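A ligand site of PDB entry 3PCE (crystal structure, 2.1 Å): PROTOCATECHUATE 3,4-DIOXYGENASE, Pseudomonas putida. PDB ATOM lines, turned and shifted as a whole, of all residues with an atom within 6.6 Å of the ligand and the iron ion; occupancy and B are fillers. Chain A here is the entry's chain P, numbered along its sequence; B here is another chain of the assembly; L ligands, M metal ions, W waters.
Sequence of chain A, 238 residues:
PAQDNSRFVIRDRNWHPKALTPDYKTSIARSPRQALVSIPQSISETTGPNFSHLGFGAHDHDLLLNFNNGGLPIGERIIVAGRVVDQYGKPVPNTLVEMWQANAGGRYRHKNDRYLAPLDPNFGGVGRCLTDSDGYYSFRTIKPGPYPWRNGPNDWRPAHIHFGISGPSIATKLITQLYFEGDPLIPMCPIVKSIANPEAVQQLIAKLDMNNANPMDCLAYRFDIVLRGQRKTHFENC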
ATOM      1  N   TYR A  24      -8.826   9.826  -5.669  1.00  0.00           N
ATOM      2  CA  TYR A  24      -8.919   9.083  -4.391  1.00  0.00           C
ATOM      3  C   TYR A  24      -7.432   8.614  -4.168  1.00  0.00           C
ATOM      4  O   TYR A  24      -7.003   7.523  -4.586  1.00  0.00           O
ATOM      5  CB  TYR A  24      -9.852   7.907  -4.488  1.00  0.00           C
ATOM      6  CG  TYR A  24      -9.931   7.025  -3.254  1.00  0.00           C
ATOM      7  CD1 TYR A  24      -9.600   7.531  -2.003  1.00  0.00           C
ATOM      8  CD2 TYR A  24     -10.414   5.721  -3.352  1.00  0.00           C
ATOM      9  CE1 TYR A  24      -9.733   6.740  -0.853  1.00  0.00           C
ATOM     10  CE2 TYR A  24     -10.540   4.883  -2.221  1.00  0.00           C
ATOM     11  CZ  TYR A  24     -10.194   5.430  -0.971  1.00  0.00           C
ATOM     12  OH  TYR A  24     -10.342   4.651   0.122  1.00  0.00           O
ATOM     13  N   THR A  26      -5.413   7.449  -1.879  1.00  0.00           N
ATOM     14  CA  THR A  26      -4.913   6.163  -1.346  1.00  0.00           C
ATOM     15  C   THR A  26      -4.881   5.005  -2.354  1.00  0.00           C
ATOM     16  O   THR A  26      -4.149   4.001  -2.157  1.00  0.00           O
ATOM     17  CB  THR A  26      -5.684   5.769  -0.002  1.00  0.00           C
ATOM     18  OG1 THR A  26      -5.291   6.815   0.951  1.00  0.00           O
ATOM     19  CG2 THR A  26      -5.147   4.417   0.572  1.00  0.00           C
ATOM     20  N   TRP A 100     -22.108  -0.962   8.950  1.00  0.00           N
ATOM     21  CA  TRP A 100     -21.377  -0.144   9.890  1.00  0.00           C
ATOM     22  C   TRP A 100     -21.519   1.324   9.423  1.00  0.00           C
ATOM     23  O   TRP A 100     -21.633   1.525   8.187  1.00  0.00           O
ATOM     24  CB  TRP A 100     -19.937  -0.552  10.217  1.00  0.00           C
ATOM     25  CG  TRP A 100     -18.894  -0.407   9.185  1.00  0.00           C
ATOM     26  CD1 TRP A 100     -17.913   0.548   9.050  1.00  0.00           C
ATOM     27  CD2 TRP A 100     -18.664  -1.349   8.094  1.00  0.00           C
ATOM     28  NE1 TRP A 100     -17.108   0.277   7.950  1.00  0.00           N
ATOM     29  CE2 TRP A 100     -17.557  -0.868   7.366  1.00  0.00           C
ATOM     30  CE3 TRP A 100     -19.339  -2.482   7.687  1.00  0.00           C
ATOM     31  CZ2 TRP A 100     -17.124  -1.510   6.190  1.00  0.00           C
ATOM     32  CZ3 TRP A 100     -18.879  -3.145   6.550  1.00  0.00           C
ATOM     33  CH2 TRP A 100     -17.786  -2.661   5.806  1.00  0.00           C
ATOM     34  N   GLN A 101     -21.461   2.226  10.373  1.00  0.00           N
ATOM     35  CA  GLN A 101     -21.571   3.682  10.003  1.00  0.00           C
ATOM     36  C   GLN A 101     -21.099   4.515  11.209  1.00  0.00           C
ATOM     37  O   GLN A 101     -20.860   3.972  12.278  1.00  0.00           O
ATOM     38  CB  GLN A 101     -23.055   4.081   9.731  1.00  0.00           C
ATOM     39  CG  GLN A 101     -23.967   3.499  10.793  1.00  0.00           C
ATOM     40  CD  GLN A 101     -25.346   4.073  10.897  1.00  0.00           C
ATOM     41  OE1 GLN A 101     -26.327   3.411  10.584  1.00  0.00           O
ATOM     42  NE2 GLN A 101     -25.523   5.328  11.353  1.00  0.00           N
ATOM     43  N   ALA A 102     -21.098   5.814  10.956  1.00  0.00           N
ATOM     44  CA  ALA A 102     -20.781   6.854  11.909  1.00  0.00           C
ATOM     45  C   ALA A 102     -22.079   7.242  12.665  1.00  0.00           C
ATOM     46  O   ALA A 102     -23.217   6.822  12.290  1.00  0.00           O
ATOM     47  CB  ALA A 102     -20.221   8.101  11.183  1.00  0.00           C
ATOM     48  N   TYR A 108     -17.052   8.116  14.091  1.00  0.00           N
ATOM     49  CA  TYR A 108     -17.043   6.613  14.142  1.00  0.00           C
ATOM     50  C   TYR A 108     -16.469   6.152  15.480  1.00  0.00           C
ATOM     51  O   TYR A 108     -15.483   6.731  15.939  1.00  0.00           O
ATOM     52  CB  TYR A 108     -16.140   6.056  13.026  1.00  0.00           C
ATOM     53  CG  TYR A 108     -16.692   5.976  11.625  1.00  0.00           C
ATOM     54  CD1 TYR A 108     -17.468   4.881  11.252  1.00  0.00           C
ATOM     55  CD2 TYR A 108     -16.438   6.948  10.659  1.00  0.00           C
ATOM     56  CE1 TYR A 108     -17.971   4.754   9.962  1.00  0.00           C
ATOM     57  CE2 TYR A 108     -16.955   6.854   9.386  1.00  0.00           C
ATOM     58  CZ  TYR A 108     -17.710   5.745   9.035  1.00  0.00           C
ATOM     59  OH  TYR A 108     -18.232   5.643   7.772  1.00  0.00           O
ATOM     60  N   TYR A 147     -18.572  13.429   6.908  1.00  0.00           N
ATOM     61  CA  TYR A 147     -17.325  13.734   7.673  1.00  0.00           C
ATOM     62  C   TYR A 147     -16.171  14.028   6.738  1.00  0.00           C
ATOM     63  O   TYR A 147     -16.103  13.600   5.579  1.00  0.00           O
ATOM     64  CB  TYR A 147     -17.070  12.689   8.762  1.00  0.00           C
ATOM     65  CG  TYR A 147     -16.893  11.343   8.084  1.00  0.00           C
ATOM     66  CD1 TYR A 147     -15.675  11.009   7.486  1.00  0.00           C
ATOM     67  CD2 TYR A 147     -17.973  10.483   7.995  1.00  0.00           C
ATOM     68  CE1 TYR A 147     -15.555   9.784   6.804  1.00  0.00           C
ATOM     69  CE2 TYR A 147     -17.856   9.247   7.333  1.00  0.00           C
ATOM     70  CZ  TYR A 147     -16.618   8.905   6.769  1.00  0.00           C
ATOM     71  OH  TYR A 147     -16.538   7.681   6.123  1.00  0.00           O
ATOM     72  N   PRO A 148     -15.272  14.860   7.263  1.00  0.00           N
ATOM     73  CA  PRO A 148     -14.071  15.326   6.522  1.00  0.00           C
ATOM     74  C   PRO A 148     -13.020  14.230   6.539  1.00  0.00           C
ATOM     75  O   PRO A 148     -13.091  13.372   7.445  1.00  0.00           O
ATOM     76  CB  PRO A 148     -13.645  16.555   7.299  1.00  0.00           C
ATOM     77  CG  PRO A 148     -14.224  16.450   8.668  1.00  0.00           C
ATOM     78  CD  PRO A 148     -15.301  15.392   8.649  1.00  0.00           C
ATOM     79  N   TRP A 149     -12.078  14.233   5.664  1.00  0.00           N
ATOM     80  CA  TRP A 149     -11.020  13.167   5.601  1.00  0.00           C
ATOM     81  C   TRP A 149      -9.862  13.816   4.841  1.00  0.00           C
ATOM     82  O   TRP A 149     -10.095  14.731   4.030  1.00  0.00           O
ATOM     83  CB  TRP A 149     -11.538  11.905   5.007  1.00  0.00           C
ATOM     84  CG  TRP A 149     -12.133  12.019   3.635  1.00  0.00           C
ATOM     85  CD1 TRP A 149     -13.139  12.841   3.180  1.00  0.00           C
ATOM     86  CD2 TRP A 149     -11.664  11.286   2.480  1.00  0.00           C
ATOM     87  NE1 TRP A 149     -13.378  12.609   1.834  1.00  0.00           N
ATOM     88  CE2 TRP A 149     -12.479  11.670   1.390  1.00  0.00           C
ATOM     89  CE3 TRP A 149     -10.649  10.345   2.299  1.00  0.00           C
ATOM     90  CZ2 TRP A 149     -12.296  11.149   0.104  1.00  0.00           C
ATOM     91  CZ3 TRP A 149     -10.475   9.806   1.043  1.00  0.00           C
ATOM     92  CH2 TRP A 149     -11.275  10.193  -0.018  1.00  0.00           C
ATOM     93  N   ARG A 150      -8.696  13.311   5.119  1.00  0.00           N
ATOM     94  CA  ARG A 150      -7.480  13.888   4.525  1.00  0.00           C
ATOM     95  C   ARG A 150      -7.239  13.327   3.128  1.00  0.00           C
ATOM     96  O   ARG A 150      -6.560  12.288   2.995  1.00  0.00           O
ATOM     97  CB  ARG A 150      -6.321  13.788   5.534  1.00  0.00           C
ATOM     98  CG  ARG A 150      -6.640  14.302   6.939  1.00  0.00           C
ATOM     99  CD  ARG A 150      -5.443  14.724   7.740  1.00  0.00           C
ATOM    100  NE  ARG A 150      -5.254  16.203   7.751  1.00  0.00           N
ATOM    101  CZ  ARG A 150      -5.483  17.012   8.803  1.00  0.00           C
ATOM    102  NH1 ARG A 150      -5.853  16.552  10.006  1.00  0.00           N
ATOM    103  NH2 ARG A 150      -5.455  18.351   8.635  1.00  0.00           N
ATOM    104  N   ARG A 157     -16.899  13.298   2.904  1.00  0.00           N
ATOM    105  CA  ARG A 157     -17.683  12.122   2.448  1.00  0.00           C
ATOM    106  C   ARG A 157     -19.163  12.499   2.678  1.00  0.00           C
ATOM    107  O   ARG A 157     -19.548  13.026   3.741  1.00  0.00           O
ATOM    108  CB  ARG A 157     -17.370  10.894   3.262  1.00  0.00           C
ATOM    109  CG  ARG A 157     -16.022  10.214   3.228  1.00  0.00           C
ATOM    110  CD  ARG A 157     -15.509   9.852   1.886  1.00  0.00           C
ATOM    111  NE  ARG A 157     -16.494   9.217   1.016  1.00  0.00           N
ATOM    112  CZ  ARG A 157     -17.174   8.102   1.095  1.00  0.00           C
ATOM    113  NH1 ARG A 157     -17.137   7.203   2.074  1.00  0.00           N
ATOM    114  NH2 ARG A 157     -18.017   7.820   0.034  1.00  0.00           N
ATOM    115  N   HIS A 160     -23.193   8.202   4.572  1.00  0.00           N
ATOM    116  CA  HIS A 160     -23.229   6.836   3.977  1.00  0.00           C
ATOM    117  C   HIS A 160     -23.215   5.721   5.016  1.00  0.00           C
ATOM    118  O   HIS A 160     -22.863   5.966   6.186  1.00  0.00           O
ATOM    119  CB  HIS A 160     -22.023   6.660   3.029  1.00  0.00           C
ATOM    120  CG  HIS A 160     -20.730   6.794   3.793  1.00  0.00           C
ATOM    121  ND1 HIS A 160     -20.075   7.942   4.035  1.00  0.00           N
ATOM    122  CD2 HIS A 160     -19.976   5.787   4.371  1.00  0.00           C
ATOM    123  CE1 HIS A 160     -18.948   7.669   4.722  1.00  0.00           C
ATOM    124  NE2 HIS A 160     -18.884   6.373   4.900  1.00  0.00           N
ATOM    125  N   HIS A 162     -21.932   1.750   5.350  1.00  0.00           N
ATOM    126  CA  HIS A 162     -21.115   0.670   4.646  1.00  0.00           C
ATOM    127  C   HIS A 162     -21.943  -0.615   4.687  1.00  0.00           C
ATOM    128  O   HIS A 162     -22.589  -0.901   5.698  1.00  0.00           O
ATOM    129  CB  HIS A 162     -19.769   0.467   5.369  1.00  0.00           C
ATOM    130  CG  HIS A 162     -18.895   1.691   5.369  1.00  0.00           C
ATOM    131  ND1 HIS A 162     -17.939   1.927   4.419  1.00  0.00           N
ATOM    132  CD2 HIS A 162     -18.849   2.761   6.163  1.00  0.00           C
ATOM    133  CE1 HIS A 162     -17.331   3.090   4.614  1.00  0.00           C
ATOM    134  NE2 HIS A 162     -17.886   3.608   5.705  1.00  0.00           N
ATOM    135  N   GLN A 177     -21.269   0.932  -0.415  1.00  0.00           N
ATOM    136  CA  GLN A 177     -21.741   2.055   0.429  1.00  0.00           C
ATOM    137  C   GLN A 177     -23.072   2.567  -0.116  1.00  0.00           C
ATOM    138  O   GLN A 177     -23.180   2.732  -1.345  1.00  0.00           O
ATOM    139  CB  GLN A 177     -20.694   3.165   0.488  1.00  0.00           C
ATOM    140  CG  GLN A 177     -19.374   2.729   1.132  1.00  0.00           C
ATOM    141  CD  GLN A 177     -18.395   3.858   1.241  1.00  0.00           C
ATOM    142  OE1 GLN A 177     -18.744   5.064   1.421  1.00  0.00           O
ATOM    143  NE2 GLN A 177     -17.108   3.569   1.038  1.00  0.00           N
ATOM    144  N   ILE A 191     -14.441   9.351  -3.979  1.00  0.00           N
ATOM    145  CA  ILE A 191     -14.708   7.923  -3.824  1.00  0.00           C
ATOM    146  C   ILE A 191     -15.910   7.542  -4.686  1.00  0.00           C
ATOM    147  O   ILE A 191     -15.850   6.555  -5.394  1.00  0.00           O
ATOM    148  CB  ILE A 191     -14.798   7.444  -2.360  1.00  0.00           C
ATOM    149  CG1 ILE A 191     -13.350   7.464  -1.743  1.00  0.00           C
ATOM    150  CG2 ILE A 191     -15.459   6.036  -2.250  1.00  0.00           C
ATOM    151  CD1 ILE A 191     -13.368   7.502  -0.187  1.00  0.00           C
ATOM    152  N   THR B  12     -14.935   0.947  -1.702  1.00  0.00           N
ATOM    153  CA  THR B  12     -13.893   0.637  -0.722  1.00  0.00           C
ATOM    154  C   THR B  12     -14.550   0.367   0.654  1.00  0.00           C
ATOM    155  O   THR B  12     -15.586   0.952   1.010  1.00  0.00           O
ATOM    156  CB  THR B  12     -12.842   1.794  -0.637  1.00  0.00           C
ATOM    157  OG1 THR B  12     -11.807   1.421   0.321  1.00  0.00           O
ATOM    158  CG2 THR B  12     -13.394   3.172  -0.296  1.00  0.00           C
ATOM    159  N   ALA B  13     -13.927  -0.548   1.396  1.00  0.00           N
ATOM    160  CA  ALA B  13     -14.344  -0.938   2.730  1.00  0.00           C
ATOM    161  C   ALA B  13     -14.070   0.239   3.681  1.00  0.00           C
ATOM    162  O   ALA B  13     -14.767   0.376   4.709  1.00  0.00           O
ATOM    163  CB  ALA B  13     -13.708  -2.262   3.161  1.00  0.00           C
ATOM    164  N   GLY B  14     -13.081   1.051   3.291  1.00  0.00           N
ATOM    165  CA  GLY B  14     -12.700   2.245   4.103  1.00  0.00           C
ATOM    166  C   GLY B  14     -11.846   1.853   5.289  1.00  0.00           C
ATOM    167  O   GLY B  14     -11.722   0.664   5.610  1.00  0.00           O
ATOM    168  N   PRO B  15     -11.279   2.873   5.978  1.00  0.00           N
ATOM    169  CA  PRO B  15     -10.405   2.692   7.137  1.00  0.00           C
ATOM    170  C   PRO B  15     -11.069   2.128   8.361  1.00  0.00           C
ATOM    171  O   PRO B  15     -10.384   1.462   9.177  1.00  0.00           O
ATOM    172  CB  PRO B  15      -9.768   4.059   7.353  1.00  0.00           C
ATOM    173  CG  PRO B  15     -10.782   5.063   6.812  1.00  0.00           C
ATOM    174  CD  PRO B  15     -11.443   4.316   5.664  1.00  0.00           C
ATOM    175  N   TYR B  16     -12.399   2.221   8.472  1.00  0.00           N
ATOM    176  CA  TYR B  16     -13.078   1.708   9.676  1.00  0.00           C
ATOM    177  C   TYR B  16     -13.792   0.420   9.501  1.00  0.00           C
ATOM    178  O   TYR B  16     -14.688   0.130  10.300  1.00  0.00           O
ATOM    179  CB  TYR B  16     -14.010   2.809  10.268  1.00  0.00           C
ATOM    180  CG  TYR B  16     -13.203   4.106  10.427  1.00  0.00           C
ATOM    181  CD1 TYR B  16     -12.056   4.151  11.205  1.00  0.00           C
ATOM    182  CD2 TYR B  16     -13.614   5.252   9.748  1.00  0.00           C
ATOM    183  CE1 TYR B  16     -11.289   5.323  11.297  1.00  0.00           C
ATOM    184  CE2 TYR B  16     -12.895   6.430   9.835  1.00  0.00           C
ATOM    185  CZ  TYR B  16     -11.733   6.469  10.616  1.00  0.00           C
ATOM    186  OH  TYR B  16     -11.058   7.654  10.654  1.00  0.00           O
ATOM    187  N   VAL B  17     -13.433  -0.345   8.492  1.00  0.00           N
ATOM    188  CA  VAL B  17     -14.044  -1.642   8.226  1.00  0.00           C
ATOM    189  C   VAL B  17     -14.145  -2.518   9.479  1.00  0.00           C
ATOM    190  O   VAL B  17     -15.119  -3.295   9.621  1.00  0.00           O
ATOM    191  CB  VAL B  17     -13.257  -2.357   7.099  1.00  0.00           C
ATOM    192  CG1 VAL B  17     -11.792  -2.556   7.430  1.00  0.00           C
ATOM    193  CG2 VAL B  17     -13.968  -3.673   6.769  1.00  0.00           C
ATOM    194  N   ARG B 133      -9.002   0.324   2.721  1.00  0.00           N
ATOM    195  CA  ARG B 133      -9.130   1.734   2.238  1.00  0.00           C
ATOM    196  C   ARG B 133      -8.071   1.839   1.108  1.00  0.00           C
ATOM    197  O   ARG B 133      -6.993   1.247   1.181  1.00  0.00           O
ATOM    198  CB  ARG B 133      -8.868   2.689   3.389  1.00  0.00           C
ATOM    199  CG  ARG B 133      -7.448   3.027   3.677  1.00  0.00           C
ATOM    200  CD  ARG B 133      -7.323   4.129   4.659  1.00  0.00           C
ATOM    201  NE  ARG B 133      -6.132   4.780   4.612  1.00  0.00           N
ATOM    202  CZ  ARG B 133      -4.893   5.009   4.761  1.00  0.00           C
ATOM    203  NH1 ARG B 133      -4.010   4.200   5.328  1.00  0.00           N
ATOM    204  NH2 ARG B 133      -4.430   6.180   4.204  1.00  0.00           N
HETATM  205  C1  LIG L   1     -10.687   8.145   4.955  1.00  0.00           C
HETATM  206  O1  LIG L   1     -10.458   8.591   6.150  1.00  0.00           O
HETATM  207  O2  LIG L   1      -9.803   7.517   4.253  1.00  0.00           O
HETATM  208  C2  LIG L   1     -12.067   8.476   4.402  1.00  0.00           C
HETATM  209  C3  LIG L   1     -13.009   7.296   4.307  1.00  0.00           C
HETATM  210  C4  LIG L   1     -13.778   6.810   5.360  1.00  0.00           C
HETATM  211  C5  LIG L   1     -14.702   5.768   5.143  1.00  0.00           C
HETATM  212  C6  LIG L   1     -14.856   5.163   3.877  1.00  0.00           C
HETATM  213  C7  LIG L   1     -14.105   5.665   2.824  1.00  0.00           C
HETATM  214  C8  LIG L   1     -13.166   6.718   3.029  1.00  0.00           C
HETATM  215  O3  LIG L   1     -15.404   5.260   6.201  1.00  0.00           O
HETATM  216 FE    FE M   1     -17.131   5.799   6.168  1.00  0.00          FE
HETATM  217  O   HOH W   1      -7.865   7.273   2.359  1.00  0.00           O
HETATM  218  O   HOH W   2      -8.718  11.156   6.863  1.00  0.00           O
HETATM  219  O   HOH W   3     -14.830   2.255   6.839  1.00  0.00           O
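Residues that only touch the ligand: Trp 149, Arg 157, Gln 177, Ile 191, Gly 14 of chain B, Pro 15 of chain B and Tyr 16 of chain B. Hydrophobic or aromatic side chains that line the ligand: Tyr 108, Tyr 147, Trp 149, His 162, Ile 191, Pro 15 of chain B and Tyr 16 of chain B. Within 4 Å of the ligand: Tyr 108, Tyr 147, Trp 149, Arg 157, His 160, His 162, Gln 177, Ile 191, Gly 14 of chain B, Pro 15 of chain B and Tyr 16 of chain B. The nearest printed residue that does not touch the ligand is Thr 12 of chain B (4.1 Å).
N of Arg 157 is in hydrogen-bond range of O of Tyr 147 (2.8 Å). The guanidinium group of Arg 157 sits close to a ring nitrogen (NE2) of His 160. N of His 162 sits at hydrogen-bond distance from O of Trp 100 (2.9 Å). The side-chain amide oxygen of Gln 177 sits at hydrogen-bond distance from the guanidinium group of Arg 157 (2.8 Å). N of Gly 14 of chain B sits close to OG1 of Thr 12 of chain B, 3.3 Å away. The side-chain amide nitrogen of Gln 177 sits at hydrogen-bond distance from the backbone carbonyl oxygen of Thr 12 of chain B. The backbone carbonyl oxygen of Tyr 16 of chain B sits at hydrogen-bond distance from the indole nitrogen of Trp 100 (3.4 Å).
The iron ion is bound by O3 of the ligand (1.8 Å), OH of Tyr 108 (2.0 Å), OH of Tyr 147 (2.0 Å), NE2 of His 160 (2.2 Å) and NE2 of His 162 (2.4 Å).
Water W1 bridges O2 of the ligand (2.7 Å) and OG1 of Thr 26 (3.0 Å). Water W2 lies within hydrogen-bond range of the backbone NH (N) of Arg 150 (2.8 Å) and an oxygen (O1) of the ligand (3.2 Å).
Of the 22 residues printed, 4 come within 4 Å of the iron ion.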
